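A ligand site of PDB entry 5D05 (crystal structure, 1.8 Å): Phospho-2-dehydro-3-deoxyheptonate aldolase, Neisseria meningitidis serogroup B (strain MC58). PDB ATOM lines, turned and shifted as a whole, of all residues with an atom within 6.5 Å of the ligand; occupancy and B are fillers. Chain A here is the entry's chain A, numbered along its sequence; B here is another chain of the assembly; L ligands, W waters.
Water W1 bridges N1 of the ligand and OD1 of Asp 8 of chain B.
Met 149 touches the ligand (O to C7, 3.6 Å). Pro 152 touches the ligand (CB to C5, 3.8 Å). CB of Ala 156 touches O1 of the ligand, 3.5 Å away. Leu 177 touches the ligand (CD1 to C5, 3.9 Å). O of Gly 180 touches C3 of the ligand, at 3.4 Å. Leu 181 touches the ligand. Phe 211 touches the ligand (CZ to C7, 3.6 Å). Ser 213 touches the ligand (OG to C9, 3.4 Å). Lys 216 touches the ligand. CG2 of Val 223 touches C8 of the ligand, 3.7 Å away. CD1 of Ile 12 of chain B touches C6 of the ligand, at 3.9 Å. Hydrophobic or aromatic side chains within 4 Å of the ligand: Pro 152, Ala 156, Leu 177, Leu 181, Phe 211, Val 223 and Ile 12 of chain B. Of the 26 residues printed, 15 come within 4 Å of the ligand. The nearest printed residue that does not touch the ligand is Thr 7 of chain B (4.2 Å).
The backbone carbonyl oxygen (O) of Leu 181 sits at hydrogen-bond distance from the side-chain amino group (NZ) of Lys 11 of chain B, 3.0 Å away. OG of Ser 213 lies within hydrogen-bond range of O of Met 149, at 2.7 Å. OD1 of Asp 8 of chain B lies within salt-bridge range of NZ of Lys 216, 2.8 Å away. The backbone carbonyl oxygen (O) of Ala 156 is in hydrogen-bond range of the guanidinium group (NH2) of Arg 42 (2.8 Å). The backbone carbonyl oxygen of Val 214 sits at hydrogen-bond distance from the side-chain amide nitrogen of Gln 153 (2.9 Å). N of Asp 9 of chain B is in hydrogen-bond range of OG of Ser 182 (3.3 Å). O of Ser 182 lies within hydrogen-bond range of NZ of Lys 11 of chain B (3.2 Å). NZ of Lys 216 sits at hydrogen-bond distance from OE1 of Gln 153.
A nitrogen (N1) of the ligand sits at hydrogen-bond distance from the side-chain amide oxygen of Gln 153, 3.0 Å away. An oxygen (O1) of the ligand lies within hydrogen-bond range of the backbone NH of Ser 182 (2.8 Å). N of Asp 9 of chain B sits at hydrogen-bond distance from O2 of the ligand. OD1 of Asp 9 of chain B lies within salt-bridge range of N1 of the ligand (2.8 Å). The side-chain carboxylate of Asp 8 of chain B lies within salt-bridge range of a nitrogen (N1) of the ligand (3.6 Å). The side-chain hydroxyl of Ser 182 is in hydrogen-bond range of an oxygen (O2) of the ligand, 2.6 Å away.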
ATOM      1  N   ARG A  42      14.408 -26.397  38.448  1.00  0.00           N
ATOM      2  CA  ARG A  42      15.428 -25.560  37.812  1.00  0.00           C
ATOM      3  C   ARG A  42      15.546 -24.174  38.472  1.00  0.00           C
ATOM      4  O   ARG A  42      16.659 -23.698  38.752  1.00  0.00           O
ATOM      5  CB  ARG A  42      15.144 -25.383  36.341  1.00  0.00           C
ATOM      6  CG  ARG A  42      15.334 -26.651  35.518  1.00  0.00           C
ATOM      7  CD  ARG A  42      14.781 -26.476  34.128  1.00  0.00           C
ATOM      8  NE  ARG A  42      15.098 -27.612  33.237  1.00  0.00           N
ATOM      9  CZ  ARG A  42      14.594 -27.735  32.022  1.00  0.00           C
ATOM     10  NH1 ARG A  42      13.743 -26.814  31.551  1.00  0.00           N
ATOM     11  NH2 ARG A  42      14.909 -28.803  31.262  1.00  0.00           N
ATOM     12  N   PHE A 146      25.563 -34.716  30.225  1.00  0.00           N
ATOM     13  CA  PHE A 146      25.445 -34.699  28.774  1.00  0.00           C
ATOM     14  C   PHE A 146      26.819 -34.903  28.123  1.00  0.00           C
ATOM     15  O   PHE A 146      27.717 -34.084  28.311  1.00  0.00           O
ATOM     16  CB  PHE A 146      24.809 -33.393  28.319  1.00  0.00           C
ATOM     17  CG  PHE A 146      23.395 -33.240  28.765  1.00  0.00           C
ATOM     18  CD1 PHE A 146      22.402 -33.970  28.180  1.00  0.00           C
ATOM     19  CD2 PHE A 146      23.071 -32.381  29.799  1.00  0.00           C
ATOM     20  CE1 PHE A 146      21.072 -33.832  28.576  1.00  0.00           C
ATOM     21  CE2 PHE A 146      21.753 -32.240  30.216  1.00  0.00           C
ATOM     22  CZ  PHE A 146      20.761 -32.958  29.599  1.00  0.00           C
ATOM     23  N   MET A 149      26.278 -33.606  21.877  1.00  0.00           N
ATOM     24  CA  MET A 149      25.496 -32.438  21.512  1.00  0.00           C
ATOM     25  C   MET A 149      24.126 -32.819  20.925  1.00  0.00           C
ATOM     26  O   MET A 149      23.317 -31.932  20.618  1.00  0.00           O
ATOM     27  CB  MET A 149      26.303 -31.571  20.523  1.00  0.00           C
ATOM     28  CG  MET A 149      27.242 -30.568  21.214  1.00  0.00           C
ATOM     29  SD  MET A 149      28.431 -31.270  22.395  1.00  0.00           S
ATOM     30  CE  MET A 149      29.367 -32.264  21.269  1.00  0.00           C
ATOM     31  N   ILE A 150      23.840 -34.109  20.850  1.00  0.00           N
ATOM     32  CA  ILE A 150      22.603 -34.625  20.192  1.00  0.00           C
ATOM     33  C   ILE A 150      21.633 -35.243  21.193  1.00  0.00           C
ATOM     34  O   ILE A 150      20.435 -34.965  21.138  1.00  0.00           O
ATOM     35  CB  ILE A 150      22.994 -35.626  19.063  1.00  0.00           C
ATOM     36  CG1 ILE A 150      23.667 -34.887  17.931  1.00  0.00           C
ATOM     37  CG2 ILE A 150      21.764 -36.432  18.550  1.00  0.00           C
ATOM     38  CD1 ILE A 150      24.358 -35.782  16.922  1.00  0.00           C
ATOM     39  N   PRO A 152      20.818 -34.403  24.195  1.00  0.00           N
ATOM     40  CA  PRO A 152      19.930 -33.495  24.912  1.00  0.00           C
ATOM     41  C   PRO A 152      18.583 -33.266  24.229  1.00  0.00           C
ATOM     42  O   PRO A 152      17.580 -33.027  24.905  1.00  0.00           O
ATOM     43  CB  PRO A 152      20.725 -32.169  24.949  1.00  0.00           C
ATOM     44  CG  PRO A 152      22.147 -32.616  24.916  1.00  0.00           C
ATOM     45  CD  PRO A 152      22.145 -33.788  23.978  1.00  0.00           C
ATOM     46  N   GLN A 153      18.550 -33.348  22.897  1.00  0.00           N
ATOM     47  CA  GLN A 153      17.316 -33.143  22.186  1.00  0.00           C
ATOM     48  C   GLN A 153      16.270 -34.216  22.473  1.00  0.00           C
ATOM     49  O   GLN A 153      15.093 -33.953  22.262  1.00  0.00           O
ATOM     50  CB  GLN A 153      17.561 -33.066  20.683  1.00  0.00           C
ATOM     51  CG  GLN A 153      18.289 -31.805  20.237  1.00  0.00           C
ATOM     52  CD  GLN A 153      17.360 -30.612  20.262  1.00  0.00           C
ATOM     53  OE1 GLN A 153      16.803 -30.281  21.324  1.00  0.00           O
ATOM     54  NE2 GLN A 153      17.129 -29.979  19.101  1.00  0.00           N
ATOM     55  N   ALA A 156      16.353 -33.595  27.390  1.00  0.00           N
ATOM     56  CA  ALA A 156      16.736 -32.453  28.265  1.00  0.00           C
ATOM     57  C   ALA A 156      15.551 -31.757  28.897  1.00  0.00           C
ATOM     58  O   ALA A 156      15.725 -31.081  29.916  1.00  0.00           O
ATOM     59  CB  ALA A 156      17.597 -31.410  27.550  1.00  0.00           C
ATOM     60  N   ASP A 157      14.387 -31.854  28.260  1.00  0.00           N
ATOM     61  CA  ASP A 157      13.164 -31.242  28.759  1.00  0.00           C
ATOM     62  C   ASP A 157      12.737 -31.853  30.080  1.00  0.00           C
ATOM     63  O   ASP A 157      11.922 -31.258  30.793  1.00  0.00           O
ATOM     64  CB  ASP A 157      12.027 -31.339  27.731  1.00  0.00           C
ATOM     65  CG  ASP A 157      11.669 -32.758  27.324  1.00  0.00           C
ATOM     66  OD1 ASP A 157      12.587 -33.562  27.003  1.00  0.00           O
ATOM     67  OD2 ASP A 157      10.457 -33.063  27.272  1.00  0.00           O
ATOM     68  N   LEU A 177      27.416 -26.156  24.058  1.00  0.00           N
ATOM     69  CA  LEU A 177      26.217 -26.878  24.510  1.00  0.00           C
ATOM     70  C   LEU A 177      25.640 -26.371  25.818  1.00  0.00           C
ATOM     71  O   LEU A 177      24.408 -26.095  25.916  1.00  0.00           O
ATOM     72  CB  LEU A 177      26.518 -28.381  24.647  1.00  0.00           C
ATOM     73  CG  LEU A 177      25.376 -29.199  25.253  1.00  0.00           C
ATOM     74  CD1 LEU A 177      24.137 -29.141  24.371  1.00  0.00           C
ATOM     75  CD2 LEU A 177      25.830 -30.647  25.447  1.00  0.00           C
ATOM     76  N   GLY A 180      23.390 -23.345  26.074  1.00  0.00           N
ATOM     77  CA  GLY A 180      22.009 -23.444  25.618  1.00  0.00           C
ATOM     78  C   GLY A 180      21.176 -24.503  26.329  1.00  0.00           C
ATOM     79  O   GLY A 180      20.057 -24.833  25.896  1.00  0.00           O
ATOM     80  N   LEU A 181      21.693 -25.063  27.415  1.00  0.00           N
ATOM     81  CA  LEU A 181      20.904 -26.076  28.159  1.00  0.00           C
ATOM     82  C   LEU A 181      19.877 -25.396  29.049  1.00  0.00           C
ATOM     83  O   LEU A 181      20.157 -24.401  29.726  1.00  0.00           O
ATOM     84  CB  LEU A 181      21.833 -27.004  28.961  1.00  0.00           C
ATOM     85  CG  LEU A 181      22.613 -28.032  28.142  1.00  0.00           C
ATOM     86  CD1 LEU A 181      23.567 -28.799  29.048  1.00  0.00           C
ATOM     87  CD2 LEU A 181      21.685 -29.037  27.444  1.00  0.00           C
ATOM     88  N   SER A 182      18.654 -25.934  29.038  1.00  0.00           N
ATOM     89  CA  SER A 182      17.546 -25.330  29.787  1.00  0.00           C
ATOM     90  C   SER A 182      17.729 -25.383  31.315  1.00  0.00           C
ATOM     91  O   SER A 182      17.141 -24.582  32.037  1.00  0.00           O
ATOM     92  CB  SER A 182      16.249 -26.008  29.388  1.00  0.00           C
ATOM     93  OG  SER A 182      15.886 -25.701  28.037  1.00  0.00           O
ATOM     94  N   CYS A 183      18.544 -26.329  31.793  1.00  0.00           N
ATOM     95  CA  CYS A 183      18.782 -26.507  33.215  1.00  0.00           C
ATOM     96  C   CYS A 183      20.071 -25.785  33.655  1.00  0.00           C
ATOM     97  O   CYS A 183      20.910 -25.447  32.831  1.00  0.00           O
ATOM     98  CB  CYS A 183      18.923 -28.008  33.515  1.00  0.00           C
ATOM     99  SG  CYS A 183      20.193 -28.795  32.466  1.00  0.00           S
ATOM    100  N   PHE A 211      26.385 -23.921  17.940  1.00  0.00           N
ATOM    101  CA  PHE A 211      26.971 -25.245  17.772  1.00  0.00           C
ATOM    102  C   PHE A 211      26.059 -26.084  16.881  1.00  0.00           C
ATOM    103  O   PHE A 211      24.909 -25.726  16.657  1.00  0.00           O
ATOM    104  CB  PHE A 211      27.254 -25.945  19.111  1.00  0.00           C
ATOM    105  CG  PHE A 211      26.017 -26.286  19.912  1.00  0.00           C
ATOM    106  CD1 PHE A 211      25.452 -25.355  20.759  1.00  0.00           C
ATOM    107  CD2 PHE A 211      25.409 -27.553  19.792  1.00  0.00           C
ATOM    108  CE1 PHE A 211      24.299 -25.665  21.507  1.00  0.00           C
ATOM    109  CE2 PHE A 211      24.264 -27.854  20.525  1.00  0.00           C
ATOM    110  CZ  PHE A 211      23.704 -26.917  21.376  1.00  0.00           C
ATOM    111  N   LEU A 212      26.597 -27.201  16.384  1.00  0.00           N
ATOM    112  CA  LEU A 212      25.839 -28.059  15.478  1.00  0.00           C
ATOM    113  C   LEU A 212      25.174 -29.191  16.227  1.00  0.00           C
ATOM    114  O   LEU A 212      25.744 -29.775  17.158  1.00  0.00           O
ATOM    115  CB  LEU A 212      26.743 -28.636  14.390  1.00  0.00           C
ATOM    116  CG  LEU A 212      27.471 -27.625  13.505  1.00  0.00           C
ATOM    117  CD1 LEU A 212      28.102 -28.261  12.272  1.00  0.00           C
ATOM    118  CD2 LEU A 212      26.521 -26.513  13.099  1.00  0.00           C
ATOM    119  N   SER A 213      23.956 -29.532  15.800  1.00  0.00           N
ATOM    120  CA  SER A 213      23.231 -30.613  16.433  1.00  0.00           C
ATOM    121  C   SER A 213      22.174 -31.025  15.416  1.00  0.00           C
ATOM    122  O   SER A 213      22.418 -30.917  14.210  1.00  0.00           O
ATOM    123  CB  SER A 213      22.631 -30.149  17.758  1.00  0.00           C
ATOM    124  OG  SER A 213      21.933 -31.189  18.424  1.00  0.00           O
ATOM    125  N   VAL A 214      21.038 -31.500  15.909  1.00  0.00           N
ATOM    126  CA  VAL A 214      19.881 -31.788  15.037  1.00  0.00           C
ATOM    127  C   VAL A 214      18.647 -31.061  15.548  1.00  0.00           C
ATOM    128  O   VAL A 214      18.554 -30.740  16.735  1.00  0.00           O
ATOM    129  CB  VAL A 214      19.573 -33.301  14.964  1.00  0.00           C
ATOM    130  CG1 VAL A 214      20.731 -34.035  14.312  1.00  0.00           C
ATOM    131  CG2 VAL A 214      19.292 -33.875  16.368  1.00  0.00           C
ATOM    132  N   LYS A 216      14.509 -31.024  16.356  1.00  0.00           N
ATOM    133  CA  LYS A 216      13.649 -32.037  16.965  1.00  0.00           C
ATOM    134  C   LYS A 216      13.178 -33.040  15.927  1.00  0.00           C
ATOM    135  O   LYS A 216      12.952 -34.220  16.268  1.00  0.00           O
ATOM    136  CB  LYS A 216      12.457 -31.398  17.688  1.00  0.00           C
ATOM    137  CG  LYS A 216      12.831 -30.610  18.938  1.00  0.00           C
ATOM    138  CD  LYS A 216      13.491 -31.478  20.011  1.00  0.00           C
ATOM    139  CE  LYS A 216      13.495 -30.796  21.373  1.00  0.00           C
ATOM    140  NZ  LYS A 216      14.156 -29.448  21.389  1.00  0.00           N
ATOM    141  N   VAL A 223      22.597 -24.432  16.076  1.00  0.00           N
ATOM    142  CA  VAL A 223      21.883 -23.987  17.271  1.00  0.00           C
ATOM    143  C   VAL A 223      22.504 -22.691  17.768  1.00  0.00           C
ATOM    144  O   VAL A 223      23.709 -22.644  17.973  1.00  0.00           O
ATOM    145  CB  VAL A 223      21.991 -25.038  18.399  1.00  0.00           C
ATOM    146  CG1 VAL A 223      21.231 -24.548  19.629  1.00  0.00           C
ATOM    147  CG2 VAL A 223      21.447 -26.350  17.910  1.00  0.00           C
ATOM    148  N   THR B   7       9.526 -26.211  29.344  1.00  0.00           N
ATOM    149  CA  THR B   7      10.820 -26.806  29.785  1.00  0.00           C
ATOM    150  C   THR B   7      11.807 -27.044  28.648  1.00  0.00           C
ATOM    151  O   THR B   7      12.942 -27.448  28.904  1.00  0.00           O
ATOM    152  CB  THR B   7      10.624 -28.125  30.515  1.00  0.00           C
ATOM    153  OG1 THR B   7      10.101 -29.077  29.598  1.00  0.00           O
ATOM    154  CG2 THR B   7       9.690 -27.970  31.725  1.00  0.00           C
ATOM    155  N   ASP B   8      11.372 -26.859  27.396  1.00  0.00           N
ATOM    156  CA  ASP B   8      12.191 -27.148  26.246  1.00  0.00           C
ATOM    157  C   ASP B   8      12.754 -25.868  25.614  1.00  0.00           C
ATOM    158  O   ASP B   8      12.005 -24.910  25.385  1.00  0.00           O
ATOM    159  CB  ASP B   8      11.353 -27.964  25.232  1.00  0.00           C
ATOM    160  CG  ASP B   8      12.067 -28.204  23.916  1.00  0.00           C
ATOM    161  OD1 ASP B   8      13.236 -28.639  23.917  1.00  0.00           O
ATOM    162  OD2 ASP B   8      11.429 -27.984  22.859  1.00  0.00           O
ATOM    163  N   ASP B   9      14.055 -25.864  25.320  1.00  0.00           N
ATOM    164  CA  ASP B   9      14.720 -24.784  24.545  1.00  0.00           C
ATOM    165  C   ASP B   9      14.581 -23.399  25.206  1.00  0.00           C
ATOM    166  O   ASP B   9      14.509 -22.355  24.548  1.00  0.00           O
ATOM    167  CB  ASP B   9      14.182 -24.746  23.096  1.00  0.00           C
ATOM    168  CG  ASP B   9      14.798 -25.815  22.197  1.00  0.00           C
ATOM    169  OD1 ASP B   9      15.560 -26.701  22.663  1.00  0.00           O
ATOM    170  OD2 ASP B   9      14.548 -25.733  20.968  1.00  0.00           O
ATOM    171  N   ILE B  10      14.582 -23.422  26.532  1.00  0.00           N
ATOM    172  CA  ILE B  10      14.380 -22.191  27.320  1.00  0.00           C
ATOM    173  C   ILE B  10      15.479 -21.187  27.002  1.00  0.00           C
ATOM    174  O   ILE B  10      15.188 -19.978  26.960  1.00  0.00           O
ATOM    175  CB  ILE B  10      14.387 -22.482  28.837  1.00  0.00           C
ATOM    176  CG1 ILE B  10      13.316 -23.526  29.199  1.00  0.00           C
ATOM    177  CG2 ILE B  10      14.202 -21.195  29.635  1.00  0.00           C
ATOM    178  CD1 ILE B  10      11.925 -23.110  28.804  1.00  0.00           C
ATOM    179  N   LYS B  11      16.719 -21.657  26.741  1.00  0.00           N
ATOM    180  CA  LYS B  11      17.876 -20.773  26.518  1.00  0.00           C
ATOM    181  C   LYS B  11      18.395 -20.841  25.086  1.00  0.00           C
ATOM    182  O   LYS B  11      19.585 -20.665  24.818  1.00  0.00           O
ATOM    183  CB  LYS B  11      18.993 -21.042  27.541  1.00  0.00           C
ATOM    184  CG  LYS B  11      18.537 -20.897  28.970  1.00  0.00           C
ATOM    185  CD  LYS B  11      19.605 -21.326  29.976  1.00  0.00           C
ATOM    186  CE  LYS B  11      18.942 -21.615  31.319  1.00  0.00           C
ATOM    187  NZ  LYS B  11      19.661 -22.631  32.117  1.00  0.00           N
ATOM    188  N   ILE B  12      17.474 -21.084  24.161  1.00  0.00           N
ATOM    189  CA  ILE B  12      17.807 -21.171  22.746  1.00  0.00           C
ATOM    190  C   ILE B  12      17.185 -20.013  21.981  1.00  0.00           C
ATOM    191  O   ILE B  12      15.957 -19.802  22.049  1.00  0.00           O
ATOM    192  CB  ILE B  12      17.301 -22.511  22.190  1.00  0.00           C
ATOM    193  CG1 ILE B  12      17.951 -23.687  22.936  1.00  0.00           C
ATOM    194  CG2 ILE B  12      17.532 -22.593  20.712  1.00  0.00           C
ATOM    195  CD1 ILE B  12      19.450 -23.805  22.746  1.00  0.00           C
ATOM    196  N   VAL B  15      17.004 -22.534  16.262  1.00  0.00           N
ATOM    197  CA  VAL B  15      17.540 -23.787  15.735  1.00  0.00           C
ATOM    198  C   VAL B  15      17.206 -23.804  14.255  1.00  0.00           C
ATOM    199  O   VAL B  15      16.003 -23.761  13.886  1.00  0.00           O
ATOM    200  CB  VAL B  15      16.923 -25.030  16.419  1.00  0.00           C
ATOM    201  CG1 VAL B  15      17.547 -26.306  15.865  1.00  0.00           C
ATOM    202  CG2 VAL B  15      17.158 -24.974  17.916  1.00  0.00           C
HETATM  203  N1  LIG L   1      16.779 -28.914  23.949  1.00  0.00           N
HETATM  204  C1  LIG L   1      17.887 -28.564  24.875  1.00  0.00           C
HETATM  205  C2  LIG L   1      17.359 -27.997  26.177  1.00  0.00           C
HETATM  206  O1  LIG L   1      18.120 -27.959  27.178  1.00  0.00           O
HETATM  207  C3  LIG L   1      18.822 -27.528  24.231  1.00  0.00           C
HETATM  208  C4  LIG L   1      19.443 -28.001  22.987  1.00  0.00           C
HETATM  209  C5  LIG L   1      20.496 -28.900  23.021  1.00  0.00           C
HETATM  210  C6  LIG L   1      18.942 -27.588  21.763  1.00  0.00           C
HETATM  211  C7  LIG L   1      21.053 -29.363  21.834  1.00  0.00           C
HETATM  212  C8  LIG L   1      19.478 -28.076  20.590  1.00  0.00           C
HETATM  213  C9  LIG L   1      20.526 -28.980  20.632  1.00  0.00           C
HETATM  214  O2  LIG L   1      16.198 -27.574  26.236  1.00  0.00           O
HETATM  215  O   HOH W   1      14.867 -30.511  25.005  1.00  0.00           O
